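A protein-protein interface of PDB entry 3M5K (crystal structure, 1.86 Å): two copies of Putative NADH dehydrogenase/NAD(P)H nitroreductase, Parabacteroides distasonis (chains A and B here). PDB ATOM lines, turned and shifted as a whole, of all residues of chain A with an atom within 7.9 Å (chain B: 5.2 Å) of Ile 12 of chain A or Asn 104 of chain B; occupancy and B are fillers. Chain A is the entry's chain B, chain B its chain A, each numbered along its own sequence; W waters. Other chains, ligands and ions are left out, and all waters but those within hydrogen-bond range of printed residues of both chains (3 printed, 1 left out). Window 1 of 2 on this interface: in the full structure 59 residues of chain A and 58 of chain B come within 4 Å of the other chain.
O of Ala 40 of chain B lies within hydrogen-bond range of NH2 of Arg 15 of chain A, at 2.9 Å.
O of Ala 40 of chain B is in hydrogen-bond range of NZ of Lys 161 of chain A (3.3 Å).
The backbone carbonyl oxygen (O) of Ala 41 of chain B sits at hydrogen-bond distance from the side-chain amino group (NZ) of Lys 161 of chain A (2.8 Å).
NE2 of Gln 103 of chain B is in hydrogen-bond range of OD1 of Asn 104 of chain A (2.8 Å).
The side-chain amide nitrogen of Gln 103 of chain A sits at hydrogen-bond distance from the side-chain amide oxygen of Asn 104 of chain B, 2.8 Å away.
O of Ala 37 of chain B is in hydrogen-bond range of ND2 of Asn 104 of chain B, at 3.0 Å.
ND2 of Asn 104 of chain B sits close to N of Ala 41 of chain B (3.3 Å).
The side-chain amide oxygen (OD1) of Asn 6 of chain A lies within hydrogen-bond range of the backbone NH (N) of Leu 9 of chain A (3.1 Å).
CD2 of Leu 9 of chain A touches CB of Ala 108 of chain B, at 3.5 Å.
Ile 12 of chain A touches Ala 37 of chain B.
Ile 12 of chain A touches Ala 40 of chain B (O to CB, 3.6 Å).
Ile 12 of chain A touches Asn 104 of chain B.
CD2 of Leu 13 of chain A touches CB of Ala 40 of chain B (3.8 Å).
Arg 15 of chain A touches Ala 41 of chain B (NH2 to C, 3.6 Å).
Ala 100 of chain B touches Gln 103 of chain A.
Asn 104 of chain A touches Leu 107 of chain B.
Leu 107 of chain A touches Asn 104 of chain B (CD1 to OD1, 3.4 Å).
CD1 of Leu 107 of chain A touches CD1 of Leu 107 of chain B (3.3 Å).
Ile 12 of chain A touches just these residues of chain B: Ala 37 (3.6 Å), Ala 40 (3.6 Å) and Asn 104 (3.6 Å).
Of the printed residues of chain A, Ala 40 of chain B touches Ile 12 (3.6 Å), Leu 13 (3.8 Å), Arg 15 (2.9 Å) and Lys 161 (3.3 Å).
Ala 101 of chain B touches none of the printed residues of chain A.
Asn 104 of chain B touches three residues of chain A.
Leu 105 of chain B touches none of the printed residues of chain A.
Printed residues of chain A within 4 Å of Leu 107 of chain B: Asn 104 (3.5 Å) and Leu 107 (3.3 Å).
The nearest residue of chain A that does not touch Asn 104 of chain B is Arg 15 of chain A (5.5 Å).
Printed residues of chain A that touch a printed residue of chain B: Leu 9, Ile 12, Leu 13, Arg 15, Ala 100, Gln 103, Asn 104, Leu 107 and Lys 161.
Of the 14 printed residues of chain B, 8 touch a printed residue of chain A.
Printed residues of chain B that touch a printed residue of chain A: Ala 37, Ala 40, Ala 41, Ala 100, Gln 103, Asn 104, Leu 107 and Ala 108.
Hydrophobic or aromatic side chains of chain B that line the printed part of chain A: Ala 40, Ala 100, Leu 107 and Ala 108.
Along chain B the printed residues that touch a printed residue of chain A span positions 37 to 108.
Among the printed residues, 16 pairs touch across the chains.
Among the printed residues, no Asp or Glu carboxylate lies within 4 Å of a Lys or Arg side-chain nitrogen of the other chain.
Ala 100 of chain A touches Gln 103 of chain B, and with the chains exchanged Gln 103 of chain A touches Ala 100 of chain B.
Gln 103 of chain A touches Asn 104 of chain B, and with the chains exchanged Asn 104 of chain A touches Gln 103 of chain B.
Asn 104 of chain A touches Leu 107 of chain B, and with the chains exchanged Leu 107 of chain A touches Asn 104 of chain B.
Leu 107 of chain A touches its own counterpart, Leu 107 of chain B.
Of the 16 pairs that touch across the chains among the printed residues, 7 have their exchanged pair printed and touching as well.
Water W2 lies within hydrogen-bond range of O of Ala 40 of chain B (2.8 Å), O of Ile 12 of chain A (2.8 Å), NE of Arg 15 of chain A (2.9 Å) and ND2 of Asn 104 of chain B (3.1 Å).
Water W3 lies within hydrogen-bond range of NZ of Lys 161 of chain A (2.8 Å), O of Lys 159 of chain A (2.8 Å) and O of Ala 40 of chain B (3.3 Å).
Water W1 lies within hydrogen-bond range of ND2 of Asn 104 of chain A (3.1 Å) and NE2 of Gln 103 of chain B (3.5 Å).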
ATOM      1  N   ASN A   6      -2.406 -18.765 -11.758  1.00  0.00           N
ATOM      2  CA  ASN A   6      -3.537 -18.114 -11.113  1.00  0.00           C
ATOM      3  C   ASN A   6      -3.025 -17.028 -10.173  1.00  0.00           C
ATOM      4  O   ASN A   6      -2.586 -17.305  -9.062  1.00  0.00           O
ATOM      5  CB  ASN A   6      -4.361 -19.179 -10.389  1.00  0.00           C
ATOM      6  CG  ASN A   6      -5.669 -18.647  -9.876  1.00  0.00           C
ATOM      7  OD1 ASN A   6      -5.760 -17.483  -9.506  1.00  0.00           O
ATOM      8  ND2 ASN A   6      -6.699 -19.498  -9.858  1.00  0.00           N
ATOM      9  N   GLN A   7      -3.044 -15.793 -10.644  1.00  0.00           N
ATOM     10  CA  GLN A   7      -2.497 -14.676  -9.883  1.00  0.00           C
ATOM     11  C   GLN A   7      -3.231 -14.408  -8.575  1.00  0.00           C
ATOM     12  O   GLN A   7      -2.617 -13.982  -7.606  1.00  0.00           O
ATOM     13  CB  GLN A   7      -2.524 -13.376 -10.698  1.00  0.00           C
ATOM     14  CG  GLN A   7      -1.398 -13.241 -11.675  1.00  0.00           C
ATOM     15  CD  GLN A   7      -1.411 -11.874 -12.374  1.00  0.00           C
ATOM     16  OE1 GLN A   7      -1.820 -10.825 -11.808  1.00  0.00           O
ATOM     17  NE2 GLN A   7      -0.973 -11.884 -13.623  1.00  0.00           N
ATOM     18  N   THR A   8      -4.543 -14.618  -8.577  1.00  0.00           N
ATOM     19  CA  THR A   8      -5.367 -14.430  -7.381  1.00  0.00           C
ATOM     20  C   THR A   8      -4.941 -15.433  -6.298  1.00  0.00           C
ATOM     21  O   THR A   8      -4.730 -15.034  -5.140  1.00  0.00           O
ATOM     22  CB  THR A   8      -6.860 -14.554  -7.706  1.00  0.00           C
ATOM     23  OG1 THR A   8      -7.207 -13.644  -8.760  1.00  0.00           O
ATOM     24  CG2 THR A   8      -7.729 -14.265  -6.461  1.00  0.00           C
ATOM     25  N   LEU A   9      -4.800 -16.715  -6.654  1.00  0.00           N
ATOM     26  CA  LEU A   9      -4.336 -17.723  -5.699  1.00  0.00           C
ATOM     27  C   LEU A   9      -2.951 -17.358  -5.203  1.00  0.00           C
ATOM     28  O   LEU A   9      -2.644 -17.473  -4.015  1.00  0.00           O
ATOM     29  CB  LEU A   9      -4.302 -19.137  -6.315  1.00  0.00           C
ATOM     30  CG  LEU A   9      -5.630 -19.820  -6.621  1.00  0.00           C
ATOM     31  CD1 LEU A   9      -5.414 -21.244  -7.226  1.00  0.00           C
ATOM     32  CD2 LEU A   9      -6.512 -19.868  -5.362  1.00  0.00           C
ATOM     33  N   GLU A  10      -2.103 -16.927  -6.129  1.00  0.00           N
ATOM     34  CA  GLU A  10      -0.755 -16.530  -5.786  1.00  0.00           C
ATOM     35  C   GLU A  10      -0.773 -15.458  -4.691  1.00  0.00           C
ATOM     36  O   GLU A  10      -0.054 -15.567  -3.697  1.00  0.00           O
ATOM     37  CB  GLU A  10       0.003 -16.058  -7.044  1.00  0.00           C
ATOM     38  CG  GLU A  10       0.277 -17.198  -8.050  1.00  0.00           C
ATOM     39  CD  GLU A  10       0.952 -16.715  -9.347  1.00  0.00           C
ATOM     40  OE1 GLU A  10       0.920 -15.499  -9.637  1.00  0.00           O
ATOM     41  OE2 GLU A  10       1.532 -17.559 -10.057  1.00  0.00           O
ATOM     42  N   THR A  11      -1.605 -14.435  -4.866  1.00  0.00           N
ATOM     43  CA  THR A  11      -1.742 -13.351  -3.876  1.00  0.00           C
ATOM     44  C   THR A  11      -2.227 -13.880  -2.522  1.00  0.00           C
ATOM     45  O   THR A  11      -1.637 -13.566  -1.479  1.00  0.00           O
ATOM     46  CB  THR A  11      -2.702 -12.246  -4.324  1.00  0.00           C
ATOM     47  OG1 THR A  11      -2.242 -11.665  -5.545  1.00  0.00           O
ATOM     48  CG2 THR A  11      -2.803 -11.152  -3.251  1.00  0.00           C
ATOM     49  N   ILE A  12      -3.235 -14.749  -2.573  1.00  0.00           N
ATOM     50  CA  ILE A  12      -3.791 -15.351  -1.362  1.00  0.00           C
ATOM     51  C   ILE A  12      -2.692 -16.099  -0.603  1.00  0.00           C
ATOM     52  O   ILE A  12      -2.550 -15.967   0.612  1.00  0.00           O
ATOM     53  CB  ILE A  12      -5.006 -16.271  -1.691  1.00  0.00           C
ATOM     54  CG1 ILE A  12      -6.218 -15.445  -2.099  1.00  0.00           C
ATOM     55  CG2 ILE A  12      -5.324 -17.188  -0.495  1.00  0.00           C
ATOM     56  CD1 ILE A  12      -7.401 -16.245  -2.677  1.00  0.00           C
ATOM     57  N   LEU A  13      -1.890 -16.866  -1.325  1.00  0.00           N
ATOM     58  CA  LEU A  13      -0.880 -17.698  -0.693  1.00  0.00           C
ATOM     59  C   LEU A  13       0.355 -16.907  -0.265  1.00  0.00           C
ATOM     60  O   LEU A  13       1.057 -17.298   0.668  1.00  0.00           O
ATOM     61  CB  LEU A  13      -0.546 -18.902  -1.610  1.00  0.00           C
ATOM     62  CG  LEU A  13      -1.730 -19.876  -1.819  1.00  0.00           C
ATOM     63  CD1 LEU A  13      -1.438 -20.910  -2.890  1.00  0.00           C
ATOM     64  CD2 LEU A  13      -2.196 -20.558  -0.515  1.00  0.00           C
ATOM     65  N   ASN A  14       0.602 -15.764  -0.895  1.00  0.00           N
ATOM     66  CA  ASN A  14       1.748 -14.930  -0.511  1.00  0.00           C
ATOM     67  C   ASN A  14       1.464 -13.796   0.429  1.00  0.00           C
ATOM     68  O   ASN A  14       2.397 -13.193   0.929  1.00  0.00           O
ATOM     69  CB  ASN A  14       2.437 -14.397  -1.747  1.00  0.00           C
ATOM     70  CG  ASN A  14       3.243 -15.464  -2.417  1.00  0.00           C
ATOM     71  OD1 ASN A  14       4.310 -15.825  -1.936  1.00  0.00           O
ATOM     72  ND2 ASN A  14       2.715 -16.024  -3.475  1.00  0.00           N
ATOM     73  N   ARG A  15       0.185 -13.518   0.713  1.00  0.00           N
ATOM     74  CA  ARG A  15      -0.150 -12.469   1.681  1.00  0.00           C
ATOM     75  C   ARG A  15       0.524 -12.792   3.005  1.00  0.00           C
ATOM     76  O   ARG A  15       0.571 -13.974   3.415  1.00  0.00           O
ATOM     77  CB  ARG A  15      -1.683 -12.349   1.869  1.00  0.00           C
ATOM     78  CG  ARG A  15      -2.149 -11.218   2.778  1.00  0.00           C
ATOM     79  CD  ARG A  15      -3.434 -11.639   3.590  1.00  0.00           C
ATOM     80  NE  ARG A  15      -3.208 -12.920   4.261  1.00  0.00           N
ATOM     81  CZ  ARG A  15      -2.468 -13.078   5.355  1.00  0.00           C
ATOM     82  NH1 ARG A  15      -1.964 -12.043   6.003  1.00  0.00           N
ATOM     83  NH2 ARG A  15      -2.265 -14.290   5.855  1.00  0.00           N
ATOM     84  N   LYS A  16       1.079 -11.759   3.647  1.00  0.00           N
ATOM     85  CA  LYS A  16       1.578 -11.831   5.009  1.00  0.00           C
ATOM     86  C   LYS A  16       1.288 -10.546   5.754  1.00  0.00           C
ATOM     87  O   LYS A  16       1.042  -9.496   5.153  1.00  0.00           O
ATOM     88  CB  LYS A  16       3.072 -12.217   5.094  1.00  0.00           C
ATOM     89  CG  LYS A  16       4.103 -11.088   4.816  1.00  0.00           C
ATOM     90  CD  LYS A  16       4.021 -10.574   3.401  1.00  0.00           C
ATOM     91  CE  LYS A  16       4.642 -11.468   2.402  1.00  0.00           C
ATOM     92  NZ  LYS A  16       4.482 -10.945   1.026  1.00  0.00           N
ATOM     93  N   ALA A 100     -14.922 -10.414   6.284  1.00  0.00           N
ATOM     94  CA  ALA A 100     -14.776 -10.686   4.843  1.00  0.00           C
ATOM     95  C   ALA A 100     -14.283  -9.442   4.081  1.00  0.00           C
ATOM     96  O   ALA A 100     -13.387  -9.534   3.231  1.00  0.00           O
ATOM     97  CB  ALA A 100     -16.123 -11.206   4.244  1.00  0.00           C
ATOM     98  N   GLN A 103     -10.596  -8.959   4.814  1.00  0.00           N
ATOM     99  CA  GLN A 103      -9.743  -9.872   4.060  1.00  0.00           C
ATOM    100  C   GLN A 103      -9.574  -9.444   2.606  1.00  0.00           C
ATOM    101  O   GLN A 103      -8.478  -9.510   2.066  1.00  0.00           O
ATOM    102  CB  GLN A 103     -10.257 -11.320   4.132  1.00  0.00           C
ATOM    103  CG  GLN A 103      -9.367 -12.372   3.469  1.00  0.00           C
ATOM    104  CD  GLN A 103      -7.958 -12.404   4.039  1.00  0.00           C
ATOM    105  OE1 GLN A 103      -7.724 -11.873   5.128  1.00  0.00           O
ATOM    106  NE2 GLN A 103      -7.011 -13.019   3.298  1.00  0.00           N
ATOM    107  N   ASN A 104     -10.642  -8.976   1.990  1.00  0.00           N
ATOM    108  CA  ASN A 104     -10.518  -8.363   0.659  1.00  0.00           C
ATOM    109  C   ASN A 104      -9.494  -7.202   0.641  1.00  0.00           C
ATOM    110  O   ASN A 104      -8.681  -7.072  -0.288  1.00  0.00           O
ATOM    111  CB  ASN A 104     -11.864  -7.815   0.209  1.00  0.00           C
ATOM    112  CG  ASN A 104     -12.756  -8.845  -0.467  1.00  0.00           C
ATOM    113  OD1 ASN A 104     -12.389 -10.007  -0.647  1.00  0.00           O
ATOM    114  ND2 ASN A 104     -13.964  -8.405  -0.856  1.00  0.00           N
ATOM    115  N   LEU A 106      -6.982  -6.655   2.826  1.00  0.00           N
ATOM    116  CA  LEU A 106      -5.634  -7.185   2.952  1.00  0.00           C
ATOM    117  C   LEU A 106      -5.083  -7.766   1.631  1.00  0.00           C
ATOM    118  O   LEU A 106      -3.918  -7.579   1.297  1.00  0.00           O
ATOM    119  CB  LEU A 106      -5.529  -8.207   4.090  1.00  0.00           C
ATOM    120  CG  LEU A 106      -5.886  -7.783   5.541  1.00  0.00           C
ATOM    121  CD1 LEU A 106      -5.830  -9.054   6.435  1.00  0.00           C
ATOM    122  CD2 LEU A 106      -4.961  -6.627   6.063  1.00  0.00           C
ATOM    123  N   LEU A 107      -5.911  -8.514   0.910  1.00  0.00           N
ATOM    124  CA  LEU A 107      -5.468  -9.099  -0.346  1.00  0.00           C
ATOM    125  C   LEU A 107      -5.188  -7.999  -1.366  1.00  0.00           C
ATOM    126  O   LEU A 107      -4.176  -8.056  -2.078  1.00  0.00           O
ATOM    127  CB  LEU A 107      -6.512 -10.091  -0.866  1.00  0.00           C
ATOM    128  CG  LEU A 107      -6.640 -11.371  -0.015  1.00  0.00           C
ATOM    129  CD1 LEU A 107      -7.893 -12.187  -0.492  1.00  0.00           C
ATOM    130  CD2 LEU A 107      -5.356 -12.193  -0.001  1.00  0.00           C
ATOM    131  N   GLU A 110      -1.758  -6.514  -0.664  1.00  0.00           N
ATOM    132  CA  GLU A 110      -0.692  -7.408  -1.145  1.00  0.00           C
ATOM    133  C   GLU A 110      -0.582  -7.350  -2.674  1.00  0.00           C
ATOM    134  O   GLU A 110       0.518  -7.322  -3.192  1.00  0.00           O
ATOM    135  CB  GLU A 110      -0.911  -8.859  -0.637  1.00  0.00           C
ATOM    136  CG  GLU A 110       0.178  -9.878  -1.029  1.00  0.00           C
ATOM    137  CD  GLU A 110       1.445  -9.804  -0.164  1.00  0.00           C
ATOM    138  OE1 GLU A 110       1.399  -9.336   0.999  1.00  0.00           O
ATOM    139  OE2 GLU A 110       2.503 -10.237  -0.663  1.00  0.00           O
ATOM    140  N   SER A 111      -1.712  -7.304  -3.379  1.00  0.00           N
ATOM    141  CA  SER A 111      -1.721  -7.246  -4.845  1.00  0.00           C
ATOM    142  C   SER A 111      -1.121  -5.980  -5.433  1.00  0.00           C
ATOM    143  O   SER A 111      -0.704  -6.002  -6.575  1.00  0.00           O
ATOM    144  CB  SER A 111      -3.132  -7.382  -5.409  1.00  0.00           C
ATOM    145  OG  SER A 111      -3.885  -6.204  -5.242  1.00  0.00           O
ATOM    146  N   PRO A 158       5.903 -15.188   3.625  1.00  0.00           N
ATOM    147  CA  PRO A 158       4.601 -15.746   4.010  1.00  0.00           C
ATOM    148  C   PRO A 158       4.766 -17.096   4.737  1.00  0.00           C
ATOM    149  O   PRO A 158       5.758 -17.816   4.532  1.00  0.00           O
ATOM    150  CB  PRO A 158       3.892 -15.951   2.685  1.00  0.00           C
ATOM    151  CG  PRO A 158       4.973 -16.167   1.728  1.00  0.00           C
ATOM    152  CD  PRO A 158       6.140 -15.335   2.187  1.00  0.00           C
ATOM    153  N   LYS A 159       3.795 -17.387   5.596  1.00  0.00           N
ATOM    154  CA  LYS A 159       3.689 -18.643   6.304  1.00  0.00           C
ATOM    155  C   LYS A 159       2.972 -19.645   5.450  1.00  0.00           C
ATOM    156  O   LYS A 159       2.017 -19.284   4.756  1.00  0.00           O
ATOM    157  CB  LYS A 159       2.869 -18.436   7.568  1.00  0.00           C
ATOM    158  CG  LYS A 159       3.545 -17.484   8.536  1.00  0.00           C
ATOM    159  CD  LYS A 159       2.714 -17.145   9.668  1.00  0.00           C
ATOM    160  CE  LYS A 159       3.420 -16.084  10.516  1.00  0.00           C
ATOM    161  NZ  LYS A 159       2.935 -16.067  11.922  1.00  0.00           N
ATOM    162  N   LYS A 161       0.585 -22.436   5.893  1.00  0.00           N
ATOM    163  CA  LYS A 161      -0.302 -22.889   6.950  1.00  0.00           C
ATOM    164  C   LYS A 161      -1.048 -24.187   6.606  1.00  0.00           C
ATOM    165  O   LYS A 161      -1.880 -24.628   7.403  1.00  0.00           O
ATOM    166  CB  LYS A 161      -1.330 -21.789   7.322  1.00  0.00           C
ATOM    167  CG  LYS A 161      -0.779 -20.421   7.708  1.00  0.00           C
ATOM    168  CD  LYS A 161      -1.776 -19.619   8.500  1.00  0.00           C
ATOM    169  CE  LYS A 161      -1.393 -18.126   8.639  1.00  0.00           C
ATOM    170  NZ  LYS A 161      -1.559 -17.350   7.373  1.00  0.00           N
ATOM    171  N   ALA B  37      -6.388 -22.255   0.033  1.00  0.00           N
ATOM    172  CA  ALA B  37      -6.675 -20.819   0.043  1.00  0.00           C
ATOM    173  C   ALA B  37      -7.231 -20.390   1.389  1.00  0.00           C
ATOM    174  O   ALA B  37      -6.735 -19.451   1.991  1.00  0.00           O
ATOM    175  CB  ALA B  37      -7.651 -20.445  -1.128  1.00  0.00           C
ATOM    176  N   GLY B  38      -8.255 -21.084   1.883  1.00  0.00           N
ATOM    177  CA  GLY B  38      -8.792 -20.797   3.218  1.00  0.00           C
ATOM    178  C   GLY B  38      -7.773 -20.804   4.334  1.00  0.00           C
ATOM    179  O   GLY B  38      -7.754 -19.920   5.188  1.00  0.00           O
ATOM    180  N   ALA B  40      -4.721 -20.158   4.216  1.00  0.00           N
ATOM    181  CA  ALA B  40      -3.771 -19.031   4.091  1.00  0.00           C
ATOM    182  C   ALA B  40      -4.246 -17.732   4.785  1.00  0.00           C
ATOM    183  O   ALA B  40      -3.535 -16.723   4.808  1.00  0.00           O
ATOM    184  CB  ALA B  40      -3.434 -18.771   2.633  1.00  0.00           C
ATOM    185  N   ALA B  41      -5.448 -17.736   5.350  1.00  0.00           N
ATOM    186  CA  ALA B  41      -5.981 -16.563   6.064  1.00  0.00           C
ATOM    187  C   ALA B  41      -5.059 -16.097   7.175  1.00  0.00           C
ATOM    188  O   ALA B  41      -4.281 -16.897   7.738  1.00  0.00           O
ATOM    189  CB  ALA B  41      -7.369 -16.875   6.665  1.00  0.00           C
ATOM    190  N   ALA B 100     -12.382 -14.685   7.496  1.00  0.00           N
ATOM    191  CA  ALA B 100     -11.280 -14.395   6.558  1.00  0.00           C
ATOM    192  C   ALA B 100     -10.932 -15.632   5.699  1.00  0.00           C
ATOM    193  O   ALA B 100     -10.731 -15.534   4.502  1.00  0.00           O
ATOM    194  CB  ALA B 100     -10.052 -13.887   7.301  1.00  0.00           C
ATOM    195  N   ALA B 101     -10.869 -16.805   6.317  1.00  0.00           N
ATOM    196  CA  ALA B 101     -10.659 -18.053   5.588  1.00  0.00           C
ATOM    197  C   ALA B 101     -11.742 -18.277   4.536  1.00  0.00           C
ATOM    198  O   ALA B 101     -11.450 -18.653   3.375  1.00  0.00           O
ATOM    199  CB  ALA B 101     -10.620 -19.233   6.597  1.00  0.00           C
ATOM    200  N   SER B 102     -12.996 -18.078   4.961  1.00  0.00           N
ATOM    201  CA  SER B 102     -14.150 -18.206   4.071  1.00  0.00           C
ATOM    202  C   SER B 102     -14.016 -17.316   2.845  1.00  0.00           C
ATOM    203  O   SER B 102     -14.259 -17.761   1.717  1.00  0.00           O
ATOM    204  CB  SER B 102     -15.456 -17.973   4.844  1.00  0.00           C
ATOM    205  OG  SER B 102     -15.651 -19.025   5.778  1.00  0.00           O
ATOM    206  N   GLN B 103     -13.659 -16.041   3.058  1.00  0.00           N
ATOM    207  CA  GLN B 103     -13.481 -15.105   1.964  1.00  0.00           C
ATOM    208  C   GLN B 103     -12.368 -15.514   0.997  1.00  0.00           C
ATOM    209  O   GLN B 103     -12.566 -15.435  -0.219  1.00  0.00           O
ATOM    210  CB  GLN B 103     -13.284 -13.653   2.501  1.00  0.00           C
ATOM    211  CG  GLN B 103     -13.266 -12.539   1.411  1.00  0.00           C
ATOM    212  CD  GLN B 103     -14.505 -12.538   0.559  1.00  0.00           C
ATOM    213  OE1 GLN B 103     -15.543 -13.092   0.954  1.00  0.00           O
ATOM    214  NE2 GLN B 103     -14.425 -11.908  -0.608  1.00  0.00           N
ATOM    215  N   ASN B 104     -11.228 -15.993   1.520  1.00  0.00           N
ATOM    216  CA  ASN B 104     -10.192 -16.581   0.645  1.00  0.00           C
ATOM    217  C   ASN B 104     -10.748 -17.711  -0.245  1.00  0.00           C
ATOM    218  O   ASN B 104     -10.415 -17.812  -1.441  1.00  0.00           O
ATOM    219  CB  ASN B 104      -9.019 -17.150   1.432  1.00  0.00           C
ATOM    220  CG  ASN B 104      -7.978 -16.116   1.839  1.00  0.00           C
ATOM    221  OD1 ASN B 104      -8.092 -14.930   1.520  1.00  0.00           O
ATOM    222  ND2 ASN B 104      -6.979 -16.577   2.615  1.00  0.00           N
ATOM    223  N   LEU B 105     -11.596 -18.550   0.358  1.00  0.00           N
ATOM    224  CA  LEU B 105     -12.149 -19.733  -0.326  1.00  0.00           C
ATOM    225  C   LEU B 105     -13.060 -19.268  -1.461  1.00  0.00           C
ATOM    226  O   LEU B 105     -12.962 -19.759  -2.600  1.00  0.00           O
ATOM    227  CB  LEU B 105     -12.866 -20.656   0.656  1.00  0.00           C
ATOM    228  CG  LEU B 105     -13.347 -22.006   0.137  1.00  0.00           C
ATOM    229  CD1 LEU B 105     -13.315 -22.982   1.315  1.00  0.00           C
ATOM    230  CD2 LEU B 105     -14.733 -21.942  -0.547  1.00  0.00           C
ATOM    231  N   LEU B 106     -13.905 -18.285  -1.186  1.00  0.00           N
ATOM    232  CA  LEU B 106     -14.824 -17.767  -2.200  1.00  0.00           C
ATOM    233  C   LEU B 106     -14.075 -17.121  -3.369  1.00  0.00           C
ATOM    234  O   LEU B 106     -14.479 -17.247  -4.539  1.00  0.00           O
ATOM    235  CB  LEU B 106     -15.794 -16.757  -1.569  1.00  0.00           C
ATOM    236  CG  LEU B 106     -16.839 -17.238  -0.526  1.00  0.00           C
ATOM    237  CD1 LEU B 106     -17.674 -16.031  -0.083  1.00  0.00           C
ATOM    238  CD2 LEU B 106     -17.766 -18.387  -1.044  1.00  0.00           C
ATOM    239  N   LEU B 107     -12.984 -16.398  -3.062  1.00  0.00           N
ATOM    240  CA  LEU B 107     -12.178 -15.769  -4.104  1.00  0.00           C
ATOM    241  C   LEU B 107     -11.448 -16.816  -4.923  1.00  0.00           C
ATOM    242  O   LEU B 107     -11.366 -16.716  -6.171  1.00  0.00           O
ATOM    243  CB  LEU B 107     -11.195 -14.773  -3.472  1.00  0.00           C
ATOM    244  CG  LEU B 107     -11.803 -13.494  -2.847  1.00  0.00           C
ATOM    245  CD1 LEU B 107     -10.715 -12.666  -2.126  1.00  0.00           C
ATOM    246  CD2 LEU B 107     -12.563 -12.639  -3.930  1.00  0.00           C
ATOM    247  N   ALA B 108     -10.878 -17.816  -4.234  1.00  0.00           N
ATOM    248  CA  ALA B 108     -10.252 -18.956  -4.904  1.00  0.00           C
ATOM    249  C   ALA B 108     -11.223 -19.599  -5.899  1.00  0.00           C
ATOM    250  O   ALA B 108     -10.858 -19.857  -7.047  1.00  0.00           O
ATOM    251  CB  ALA B 108      -9.719 -19.972  -3.900  1.00  0.00           C
ATOM    252  N   ALA B 109     -12.450 -19.864  -5.464  1.00  0.00           N
ATOM    253  CA  ALA B 109     -13.484 -20.426  -6.334  1.00  0.00           C
ATOM    254  C   ALA B 109     -13.703 -19.575  -7.582  1.00  0.00           C
ATOM    255  O   ALA B 109     -13.599 -20.075  -8.707  1.00  0.00           O
ATOM    256  CB  ALA B 109     -14.816 -20.626  -5.559  1.00  0.00           C
HETATM  257  O   HOH W   1     -15.468  -9.818  -3.209  1.00  0.00           O
HETATM  258  O   HOH W   2      -4.255 -15.108   2.669  1.00  0.00           O
HETATM  259  O   HOH W   3      -0.523 -18.101   4.899  1.00  0.00           O
